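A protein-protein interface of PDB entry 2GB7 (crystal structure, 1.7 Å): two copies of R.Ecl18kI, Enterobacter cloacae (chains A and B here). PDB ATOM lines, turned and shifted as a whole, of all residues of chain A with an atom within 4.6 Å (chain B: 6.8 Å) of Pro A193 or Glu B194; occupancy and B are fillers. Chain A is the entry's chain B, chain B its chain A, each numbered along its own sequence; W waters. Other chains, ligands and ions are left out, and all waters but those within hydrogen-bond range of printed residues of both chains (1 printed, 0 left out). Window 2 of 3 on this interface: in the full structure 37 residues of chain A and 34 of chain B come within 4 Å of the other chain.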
ATOM      1  N   TRP A 189      -7.506 -15.051  12.179  1.00  0.00           N
ATOM      2  CA  TRP A 189      -6.129 -15.300  11.730  1.00  0.00           C
ATOM      3  C   TRP A 189      -5.260 -14.035  11.739  1.00  0.00           C
ATOM      4  O   TRP A 189      -4.063 -14.125  11.831  1.00  0.00           O
ATOM      5  CB  TRP A 189      -6.083 -15.936  10.334  1.00  0.00           C
ATOM      6  CG  TRP A 189      -6.713 -15.082   9.278  1.00  0.00           C
ATOM      7  CD1 TRP A 189      -7.992 -15.171   8.821  1.00  0.00           C
ATOM      8  CD2 TRP A 189      -6.106 -13.982   8.569  1.00  0.00           C
ATOM      9  NE1 TRP A 189      -8.224 -14.210   7.859  1.00  0.00           N
ATOM     10  CE2 TRP A 189      -7.076 -13.472   7.684  1.00  0.00           C
ATOM     11  CE3 TRP A 189      -4.829 -13.393   8.591  1.00  0.00           C
ATOM     12  CZ2 TRP A 189      -6.831 -12.373   6.845  1.00  0.00           C
ATOM     13  CZ3 TRP A 189      -4.573 -12.305   7.750  1.00  0.00           C
ATOM     14  CH2 TRP A 189      -5.545 -11.819   6.876  1.00  0.00           C
ATOM     15  N   GLN A 190      -5.896 -12.873  11.616  1.00  0.00           N
ATOM     16  CA  GLN A 190      -5.184 -11.603  11.614  1.00  0.00           C
ATOM     17  C   GLN A 190      -4.409 -11.400  12.909  1.00  0.00           C
ATOM     18  O   GLN A 190      -3.427 -10.640  12.930  1.00  0.00           O
ATOM     19  CB  GLN A 190      -6.187 -10.467  11.384  1.00  0.00           C
ATOM     20  CG  GLN A 190      -6.803 -10.503   9.951  1.00  0.00           C
ATOM     21  CD  GLN A 190      -8.025  -9.584   9.778  1.00  0.00           C
ATOM     22  OE1 GLN A 190      -8.471  -8.950  10.727  1.00  0.00           O
ATOM     23  NE2 GLN A 190      -8.623  -9.604   8.588  1.00  0.00           N
ATOM     24  N   GLU A 191      -4.820 -12.090  13.988  1.00  0.00           N
ATOM     25  CA  GLU A 191      -4.109 -11.988  15.279  1.00  0.00           C
ATOM     26  C   GLU A 191      -2.699 -12.546  15.171  1.00  0.00           C
ATOM     27  O   GLU A 191      -1.811 -12.143  15.922  1.00  0.00           O
ATOM     28  CB  GLU A 191      -4.874 -12.747  16.358  1.00  0.00           C
ATOM     29  CG  GLU A 191      -6.301 -12.153  16.566  1.00  0.00           C
ATOM     30  CD  GLU A 191      -7.190 -13.008  17.459  1.00  0.00           C
ATOM     31  OE1 GLU A 191      -6.722 -14.103  17.884  1.00  0.00           O
ATOM     32  OE2 GLU A 191      -8.381 -12.592  17.710  1.00  0.00           O
ATOM     33  N   VAL A 192      -2.519 -13.506  14.266  1.00  0.00           N
ATOM     34  CA  VAL A 192      -1.257 -14.255  14.214  1.00  0.00           C
ATOM     35  C   VAL A 192      -0.106 -13.388  13.664  1.00  0.00           C
ATOM     36  O   VAL A 192       0.898 -13.293  14.348  1.00  0.00           O
ATOM     37  CB  VAL A 192      -1.414 -15.619  13.496  1.00  0.00           C
ATOM     38  CG1 VAL A 192      -0.137 -16.401  13.616  1.00  0.00           C
ATOM     39  CG2 VAL A 192      -2.557 -16.424  14.155  1.00  0.00           C
ATOM     40  N   PRO A 193      -0.271 -12.735  12.486  1.00  0.00           N
ATOM     41  CA  PRO A 193       0.783 -11.818  12.037  1.00  0.00           C
ATOM     42  C   PRO A 193       1.053 -10.712  13.047  1.00  0.00           C
ATOM     43  O   PRO A 193       2.171 -10.273  13.196  1.00  0.00           O
ATOM     44  CB  PRO A 193       0.203 -11.223  10.748  1.00  0.00           C
ATOM     45  CG  PRO A 193      -0.639 -12.270  10.189  1.00  0.00           C
ATOM     46  CD  PRO A 193      -1.342 -12.788  11.475  1.00  0.00           C
ATOM     47  N   GLU A 194       0.027 -10.258  13.759  1.00  0.00           N
ATOM     48  CA  GLU A 194       0.276  -9.236  14.764  1.00  0.00           C
ATOM     49  C   GLU A 194       1.269  -9.731  15.802  1.00  0.00           C
ATOM     50  O   GLU A 194       2.227  -9.020  16.142  1.00  0.00           O
ATOM     51  CB  GLU A 194      -1.052  -8.783  15.413  1.00  0.00           C
ATOM     52  CG  GLU A 194      -0.804  -7.655  16.433  1.00  0.00           C
ATOM     53  CD  GLU A 194      -0.338  -8.112  17.793  1.00  0.00           C
ATOM     54  OE1 GLU A 194      -0.675  -9.244  18.224  1.00  0.00           O
ATOM     55  OE2 GLU A 194       0.350  -7.291  18.470  1.00  0.00           O
ATOM     56  N   GLU A 195       1.099 -10.964  16.261  1.00  0.00           N
ATOM     57  CA  GLU A 195       1.992 -11.505  17.269  1.00  0.00           C
ATOM     58  C   GLU A 195       3.369 -11.841  16.697  1.00  0.00           C
ATOM     59  O   GLU A 195       4.375 -11.569  17.345  1.00  0.00           O
ATOM     60  CB  GLU A 195       1.359 -12.690  17.993  1.00  0.00           C
ATOM     61  CG  GLU A 195       0.243 -12.198  18.922  1.00  0.00           C
ATOM     62  CD  GLU A 195       0.826 -11.348  20.057  1.00  0.00           C
ATOM     63  OE1 GLU A 195       1.527 -11.923  20.915  1.00  0.00           O
ATOM     64  OE2 GLU A 195       0.617 -10.118  20.091  1.00  0.00           O
ATOM     65  N   VAL A 196       3.399 -12.337  15.465  1.00  0.00           N
ATOM     66  CA  VAL A 196       4.685 -12.616  14.797  1.00  0.00           C
ATOM     67  C   VAL A 196       5.489 -11.346  14.669  1.00  0.00           C
ATOM     68  O   VAL A 196       6.677 -11.283  15.049  1.00  0.00           O
ATOM     69  CB  VAL A 196       4.434 -13.263  13.445  1.00  0.00           C
ATOM     70  CG1 VAL A 196       5.714 -13.306  12.583  1.00  0.00           C
ATOM     71  CG2 VAL A 196       3.993 -14.679  13.667  1.00  0.00           C
ATOM     72  N   ASN A 197       4.841 -10.299  14.182  1.00  0.00           N
ATOM     73  CA  ASN A 197       5.571  -9.059  13.961  1.00  0.00           C
ATOM     74  C   ASN A 197       5.965  -8.343  15.245  1.00  0.00           C
ATOM     75  O   ASN A 197       7.032  -7.703  15.304  1.00  0.00           O
ATOM     76  CB  ASN A 197       4.792  -8.186  13.007  1.00  0.00           C
ATOM     77  CG  ASN A 197       4.777  -8.760  11.600  1.00  0.00           C
ATOM     78  OD1 ASN A 197       3.781  -8.648  10.884  1.00  0.00           O
ATOM     79  ND2 ASN A 197       5.868  -9.393  11.204  1.00  0.00           N
ATOM     80  N   ILE A 220      -1.575 -13.576   2.477  1.00  0.00           N
ATOM     81  CA  ILE A 220      -1.201 -12.589   3.505  1.00  0.00           C
ATOM     82  C   ILE A 220      -0.443 -13.275   4.630  1.00  0.00           C
ATOM     83  O   ILE A 220       0.579 -12.765   5.087  1.00  0.00           O
ATOM     84  CB  ILE A 220      -2.451 -11.885   4.068  1.00  0.00           C
ATOM     85  CG1 ILE A 220      -3.075 -11.024   2.979  1.00  0.00           C
ATOM     86  CG2 ILE A 220      -2.102 -11.105   5.319  1.00  0.00           C
ATOM     87  CD1 ILE A 220      -4.497 -10.544   3.289  1.00  0.00           C
ATOM     88  N   LEU A 221      -0.909 -14.448   5.050  1.00  0.00           N
ATOM     89  CA  LEU A 221      -0.192 -15.211   6.066  1.00  0.00           C
ATOM     90  C   LEU A 221       1.227 -15.554   5.585  1.00  0.00           C
ATOM     91  O   LEU A 221       2.178 -15.462   6.341  1.00  0.00           O
ATOM     92  CB  LEU A 221      -0.974 -16.494   6.436  1.00  0.00           C
ATOM     93  CG  LEU A 221      -2.238 -16.150   7.227  1.00  0.00           C
ATOM     94  CD1 LEU A 221      -3.015 -17.436   7.346  1.00  0.00           C
ATOM     95  CD2 LEU A 221      -1.893 -15.574   8.618  1.00  0.00           C
ATOM     96  N   ALA A 224       3.614 -12.921   5.912  1.00  0.00           N
ATOM     97  CA  ALA A 224       3.864 -12.776   7.344  1.00  0.00           C
ATOM     98  C   ALA A 224       4.640 -13.937   7.963  1.00  0.00           C
ATOM     99  O   ALA A 224       4.900 -13.934   9.177  1.00  0.00           O
ATOM    100  CB  ALA A 224       2.531 -12.532   8.098  1.00  0.00           C
ATOM    101  N   VAL A 226       3.649 -16.982   8.304  1.00  0.00           N
ATOM    102  CA  VAL A 226       2.753 -17.867   9.036  1.00  0.00           C
ATOM    103  C   VAL A 226       2.289 -18.920   8.046  1.00  0.00           C
ATOM    104  O   VAL A 226       1.824 -18.576   6.957  1.00  0.00           O
ATOM    105  CB  VAL A 226       1.531 -17.099   9.571  1.00  0.00           C
ATOM    106  CG1 VAL A 226       0.562 -18.055  10.232  1.00  0.00           C
ATOM    107  CG2 VAL A 226       1.963 -16.052  10.598  1.00  0.00           C
ATOM    108  N   LEU B 158     -11.656  -3.782   7.874  1.00  0.00           N
ATOM    109  CA  LEU B 158     -11.720  -3.470   9.305  1.00  0.00           C
ATOM    110  C   LEU B 158     -11.930  -1.949   9.472  1.00  0.00           C
ATOM    111  O   LEU B 158     -12.505  -1.496  10.467  1.00  0.00           O
ATOM    112  CB  LEU B 158     -10.447  -4.065   9.960  1.00  0.00           C
ATOM    113  CG  LEU B 158      -9.930  -3.645  11.331  1.00  0.00           C
ATOM    114  CD1 LEU B 158      -9.422  -4.857  12.095  1.00  0.00           C
ATOM    115  CD2 LEU B 158      -8.828  -2.615  11.202  1.00  0.00           C
ATOM    116  N   TRP B 189      -8.501  -6.965  19.373  1.00  0.00           N
ATOM    117  CA  TRP B 189      -7.730  -5.788  19.020  1.00  0.00           C
ATOM    118  C   TRP B 189      -6.471  -6.091  18.221  1.00  0.00           C
ATOM    119  O   TRP B 189      -5.996  -5.253  17.455  1.00  0.00           O
ATOM    120  CB  TRP B 189      -7.357  -5.000  20.272  1.00  0.00           C
ATOM    121  CG  TRP B 189      -6.529  -5.764  21.242  1.00  0.00           C
ATOM    122  CD1 TRP B 189      -6.978  -6.423  22.347  1.00  0.00           C
ATOM    123  CD2 TRP B 189      -5.104  -5.935  21.226  1.00  0.00           C
ATOM    124  NE1 TRP B 189      -5.922  -7.020  23.008  1.00  0.00           N
ATOM    125  CE2 TRP B 189      -4.767  -6.724  22.349  1.00  0.00           C
ATOM    126  CE3 TRP B 189      -4.082  -5.513  20.368  1.00  0.00           C
ATOM    127  CZ2 TRP B 189      -3.452  -7.116  22.628  1.00  0.00           C
ATOM    128  CZ3 TRP B 189      -2.770  -5.911  20.649  1.00  0.00           C
ATOM    129  CH2 TRP B 189      -2.473  -6.676  21.775  1.00  0.00           C
ATOM    130  N   GLN B 190      -5.970  -7.310  18.372  1.00  0.00           N
ATOM    131  CA  GLN B 190      -4.742  -7.721  17.666  1.00  0.00           C
ATOM    132  C   GLN B 190      -4.912  -7.694  16.139  1.00  0.00           C
ATOM    133  O   GLN B 190      -3.935  -7.592  15.403  1.00  0.00           O
ATOM    134  CB  GLN B 190      -4.301  -9.111  18.132  1.00  0.00           C
ATOM    135  CG  GLN B 190      -3.897  -9.143  19.614  1.00  0.00           C
ATOM    136  CD  GLN B 190      -3.825 -10.543  20.163  1.00  0.00           C
ATOM    137  OE1 GLN B 190      -3.438 -10.753  21.308  1.00  0.00           O
ATOM    138  NE2 GLN B 190      -4.168 -11.510  19.346  1.00  0.00           N
ATOM    139  N   GLU B 191      -6.177  -7.740  15.676  1.00  0.00           N
ATOM    140  CA  GLU B 191      -6.467  -7.644  14.252  1.00  0.00           C
ATOM    141  C   GLU B 191      -6.057  -6.301  13.678  1.00  0.00           C
ATOM    142  O   GLU B 191      -5.741  -6.181  12.509  1.00  0.00           O
ATOM    143  CB  GLU B 191      -7.980  -7.895  14.029  1.00  0.00           C
ATOM    144  CG  GLU B 191      -8.381  -9.274  14.479  1.00  0.00           C
ATOM    145  CD  GLU B 191      -9.888  -9.489  14.459  1.00  0.00           C
ATOM    146  OE1 GLU B 191     -10.570  -8.539  14.088  1.00  0.00           O
ATOM    147  OE2 GLU B 191     -10.337 -10.631  14.771  1.00  0.00           O
ATOM    148  N   VAL B 192      -6.116  -5.273  14.505  1.00  0.00           N
ATOM    149  CA  VAL B 192      -5.960  -3.913  14.011  1.00  0.00           C
ATOM    150  C   VAL B 192      -4.492  -3.615  13.618  1.00  0.00           C
ATOM    151  O   VAL B 192      -4.267  -3.164  12.504  1.00  0.00           O
ATOM    152  CB  VAL B 192      -6.531  -2.899  14.972  1.00  0.00           C
ATOM    153  CG1 VAL B 192      -6.544  -1.532  14.326  1.00  0.00           C
ATOM    154  CG2 VAL B 192      -8.002  -3.279  15.388  1.00  0.00           C
ATOM    155  N   PRO B 193      -3.515  -3.869  14.511  1.00  0.00           N
ATOM    156  CA  PRO B 193      -2.126  -3.671  14.072  1.00  0.00           C
ATOM    157  C   PRO B 193      -1.791  -4.495  12.840  1.00  0.00           C
ATOM    158  O   PRO B 193      -0.983  -4.080  12.014  1.00  0.00           O
ATOM    159  CB  PRO B 193      -1.311  -4.161  15.279  1.00  0.00           C
ATOM    160  CG  PRO B 193      -2.202  -3.859  16.437  1.00  0.00           C
ATOM    161  CD  PRO B 193      -3.558  -4.258  15.932  1.00  0.00           C
ATOM    162  N   GLU B 194      -2.381  -5.686  12.700  1.00  0.00           N
ATOM    163  CA  GLU B 194      -2.137  -6.470  11.512  1.00  0.00           C
ATOM    164  C   GLU B 194      -2.516  -5.714  10.246  1.00  0.00           C
ATOM    165  O   GLU B 194      -1.751  -5.708   9.272  1.00  0.00           O
ATOM    166  CB  GLU B 194      -2.845  -7.822  11.584  1.00  0.00           C
ATOM    167  CG  GLU B 194      -2.493  -8.742  10.416  1.00  0.00           C
ATOM    168  CD  GLU B 194      -3.300  -8.479   9.162  1.00  0.00           C
ATOM    169  OE1 GLU B 194      -4.454  -7.993   9.281  1.00  0.00           O
ATOM    170  OE2 GLU B 194      -2.796  -8.806   8.057  1.00  0.00           O
ATOM    171  N   GLU B 195      -3.675  -5.037  10.291  1.00  0.00           N
ATOM    172  CA  GLU B 195      -4.163  -4.336   9.113  1.00  0.00           C
ATOM    173  C   GLU B 195      -3.373  -3.055   8.905  1.00  0.00           C
ATOM    174  O   GLU B 195      -3.031  -2.698   7.759  1.00  0.00           O
ATOM    175  CB  GLU B 195      -5.651  -4.102   9.258  1.00  0.00           C
ATOM    176  CG  GLU B 195      -6.404  -5.397   9.028  1.00  0.00           C
ATOM    177  CD  GLU B 195      -6.231  -5.865   7.608  1.00  0.00           C
ATOM    178  OE1 GLU B 195      -6.589  -5.081   6.714  1.00  0.00           O
ATOM    179  OE2 GLU B 195      -5.680  -6.983   7.377  1.00  0.00           O
ATOM    180  N   VAL B 196      -2.994  -2.439  10.008  1.00  0.00           N
ATOM    181  CA  VAL B 196      -2.190  -1.213   9.933  1.00  0.00           C
ATOM    182  C   VAL B 196      -0.856  -1.502   9.254  1.00  0.00           C
ATOM    183  O   VAL B 196      -0.485  -0.843   8.274  1.00  0.00           O
ATOM    184  CB  VAL B 196      -2.002  -0.544  11.325  1.00  0.00           C
ATOM    185  CG1 VAL B 196      -0.934   0.550  11.267  1.00  0.00           C
ATOM    186  CG2 VAL B 196      -3.316   0.072  11.812  1.00  0.00           C
ATOM    187  N   ASN B 197      -0.158  -2.537   9.719  1.00  0.00           N
ATOM    188  CA  ASN B 197       1.150  -2.914   9.158  1.00  0.00           C
ATOM    189  C   ASN B 197       1.097  -3.460   7.728  1.00  0.00           C
ATOM    190  O   ASN B 197       1.997  -3.224   6.899  1.00  0.00           O
ATOM    191  CB  ASN B 197       1.863  -3.808  10.173  1.00  0.00           C
ATOM    192  CG  ASN B 197       2.289  -3.015  11.418  1.00  0.00           C
ATOM    193  OD1 ASN B 197       2.872  -1.932  11.302  1.00  0.00           O
ATOM    194  ND2 ASN B 197       1.975  -3.526  12.595  1.00  0.00           N
ATOM    195  N   ARG B 198       0.011  -4.137   7.402  1.00  0.00           N
ATOM    196  CA  ARG B 198      -0.127  -4.744   6.098  1.00  0.00           C
ATOM    197  C   ARG B 198      -0.196  -3.703   4.970  1.00  0.00           C
ATOM    198  O   ARG B 198       0.346  -3.923   3.875  1.00  0.00           O
ATOM    199  CB  ARG B 198      -1.363  -5.670   6.088  1.00  0.00           C
ATOM    200  CG  ARG B 198      -1.545  -6.470   4.826  1.00  0.00           C
ATOM    201  CD  ARG B 198      -2.684  -7.417   4.954  1.00  0.00           C
ATOM    202  NE  ARG B 198      -3.954  -6.718   4.916  1.00  0.00           N
ATOM    203  CZ  ARG B 198      -4.531  -6.239   3.816  1.00  0.00           C
ATOM    204  NH1 ARG B 198      -3.947  -6.372   2.628  1.00  0.00           N
ATOM    205  NH2 ARG B 198      -5.701  -5.606   3.924  1.00  0.00           N
ATOM    206  N   THR B 199      -0.849  -2.575   5.255  1.00  0.00           N
ATOM    207  CA  THR B 199      -1.160  -1.607   4.212  1.00  0.00           C
ATOM    208  C   THR B 199      -0.422  -0.277   4.376  1.00  0.00           C
ATOM    209  O   THR B 199      -0.679   0.663   3.618  1.00  0.00           O
ATOM    210  CB  THR B 199      -2.672  -1.327   4.158  1.00  0.00           C
ATOM    211  OG1 THR B 199      -3.094  -0.808   5.409  1.00  0.00           O
ATOM    212  CG2 THR B 199      -3.443  -2.635   3.893  1.00  0.00           C
ATOM    213  N   ALA B 224       1.950   0.399  17.664  1.00  0.00           N
ATOM    214  CA  ALA B 224       1.404   0.088  16.359  1.00  0.00           C
ATOM    215  C   ALA B 224       0.662   1.229  15.703  1.00  0.00           C
ATOM    216  O   ALA B 224       0.149   1.093  14.606  1.00  0.00           O
ATOM    217  CB  ALA B 224       0.548  -1.161  16.432  1.00  0.00           C
HETATM  218  O   HOH W   1     -11.055  -7.875  10.696  1.00  0.00           O
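Water W1 lies within hydrogen-bond range of the side-chain amide oxygen (OE1) of Gln A190 (2.8 Å) and the side-chain carboxylate (OE1) of Glu B191 (3.5 Å).
CZ3 of Trp A189 touches OE2 of Glu B194 (3.9 Å).
O of Gln A190 touches O of Gln B190, at 3.96 Å.
Glu B191 touches Gln A190 (CB to OE1, 3.5 Å).
Gln A190 touches Glu B194 (O to CB, 3.2 Å).
Glu A191 touches Gln B190 (CB to NE2, 3.3 Å).
Pro A193 touches Glu B194 (CB to CG, 3.7 Å).
CB of Glu A194 touches O of Gln B190 (3.1 Å).
Glu A194 touches Pro B193.
Ile A220 touches Glu B194.
Arg B198 touches Ile A220.
Printed residues of chain B that touch a printed residue of chain A: Gln B190, Glu B191, Pro B193, Glu B194 and Arg B198.
Hydrophobic or aromatic side chains of chain B that line the printed part of chain A: Pro B193.
Printed residues of chain A that touch a printed residue of chain B: Trp A189, Gln A190, Glu A191, Pro A193, Glu A194 and Ile A220.
Hydrophobic or aromatic side chains of chain A within 4 Å of the printed part of chain B: Trp A189, Pro A193 and Ile A220.
Among the printed residues, no Asp or Glu carboxylate lies within 4 Å of a Lys or Arg side-chain nitrogen of the other chain.
Trp A189 touches Glu B194, but with the chains exchanged Glu A194 does not touch Trp B189 (4.05 Å).
Gln B190 touches its own counterpart, Gln A190.
Gln A190 touches Glu B191, and with the chains exchanged Glu A191 touches Gln B190.
Gln A190 touches Glu B194, and with the chains exchanged Glu A194 touches Gln B190.
Of the 10 pairs that touch across the chains among the printed residues, 7 have their exchanged pair printed and touching as well.
Printed residues of chain B within 4 Å of Pro A193: Glu B194 (3.7 Å).
Of chain A, only Trp A189 (3.9 Å), Gln A190 (3.2 Å), Pro A193 (3.7 Å) and Ile A220 (3.6 Å) come within 4 Å of Glu B194.
Printed residues of chain B within 4 Å of Glu A191: Gln B190 (3.3 Å).
Printed residues of chain B within 4 Å of Ile A220: Glu B194 (3.6 Å) and Arg B198 (3.8 Å).
Of the printed residues of chain A, Pro B193 touches Glu A194.
Leu A221 touches none of the printed residues of chain B.
OE2 of Glu A195 sits close to OE1 of Glu A194 (2.4 Å).
OD1 of Asn A197 sits close to O of Pro A193 (3.3 Å).
OE1 of Glu B195 lies within salt-bridge range of NH2 of Arg B198 (3.0 Å).
O of Pro B193 lies within hydrogen-bond range of ND2 of Asn B197.
OE1 of Glu B194 lies close to OE2 of Glu B195 (2.5 Å).
The guanidinium group of Arg B198 is in salt-bridge range of the side-chain carboxylate of Glu B194.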
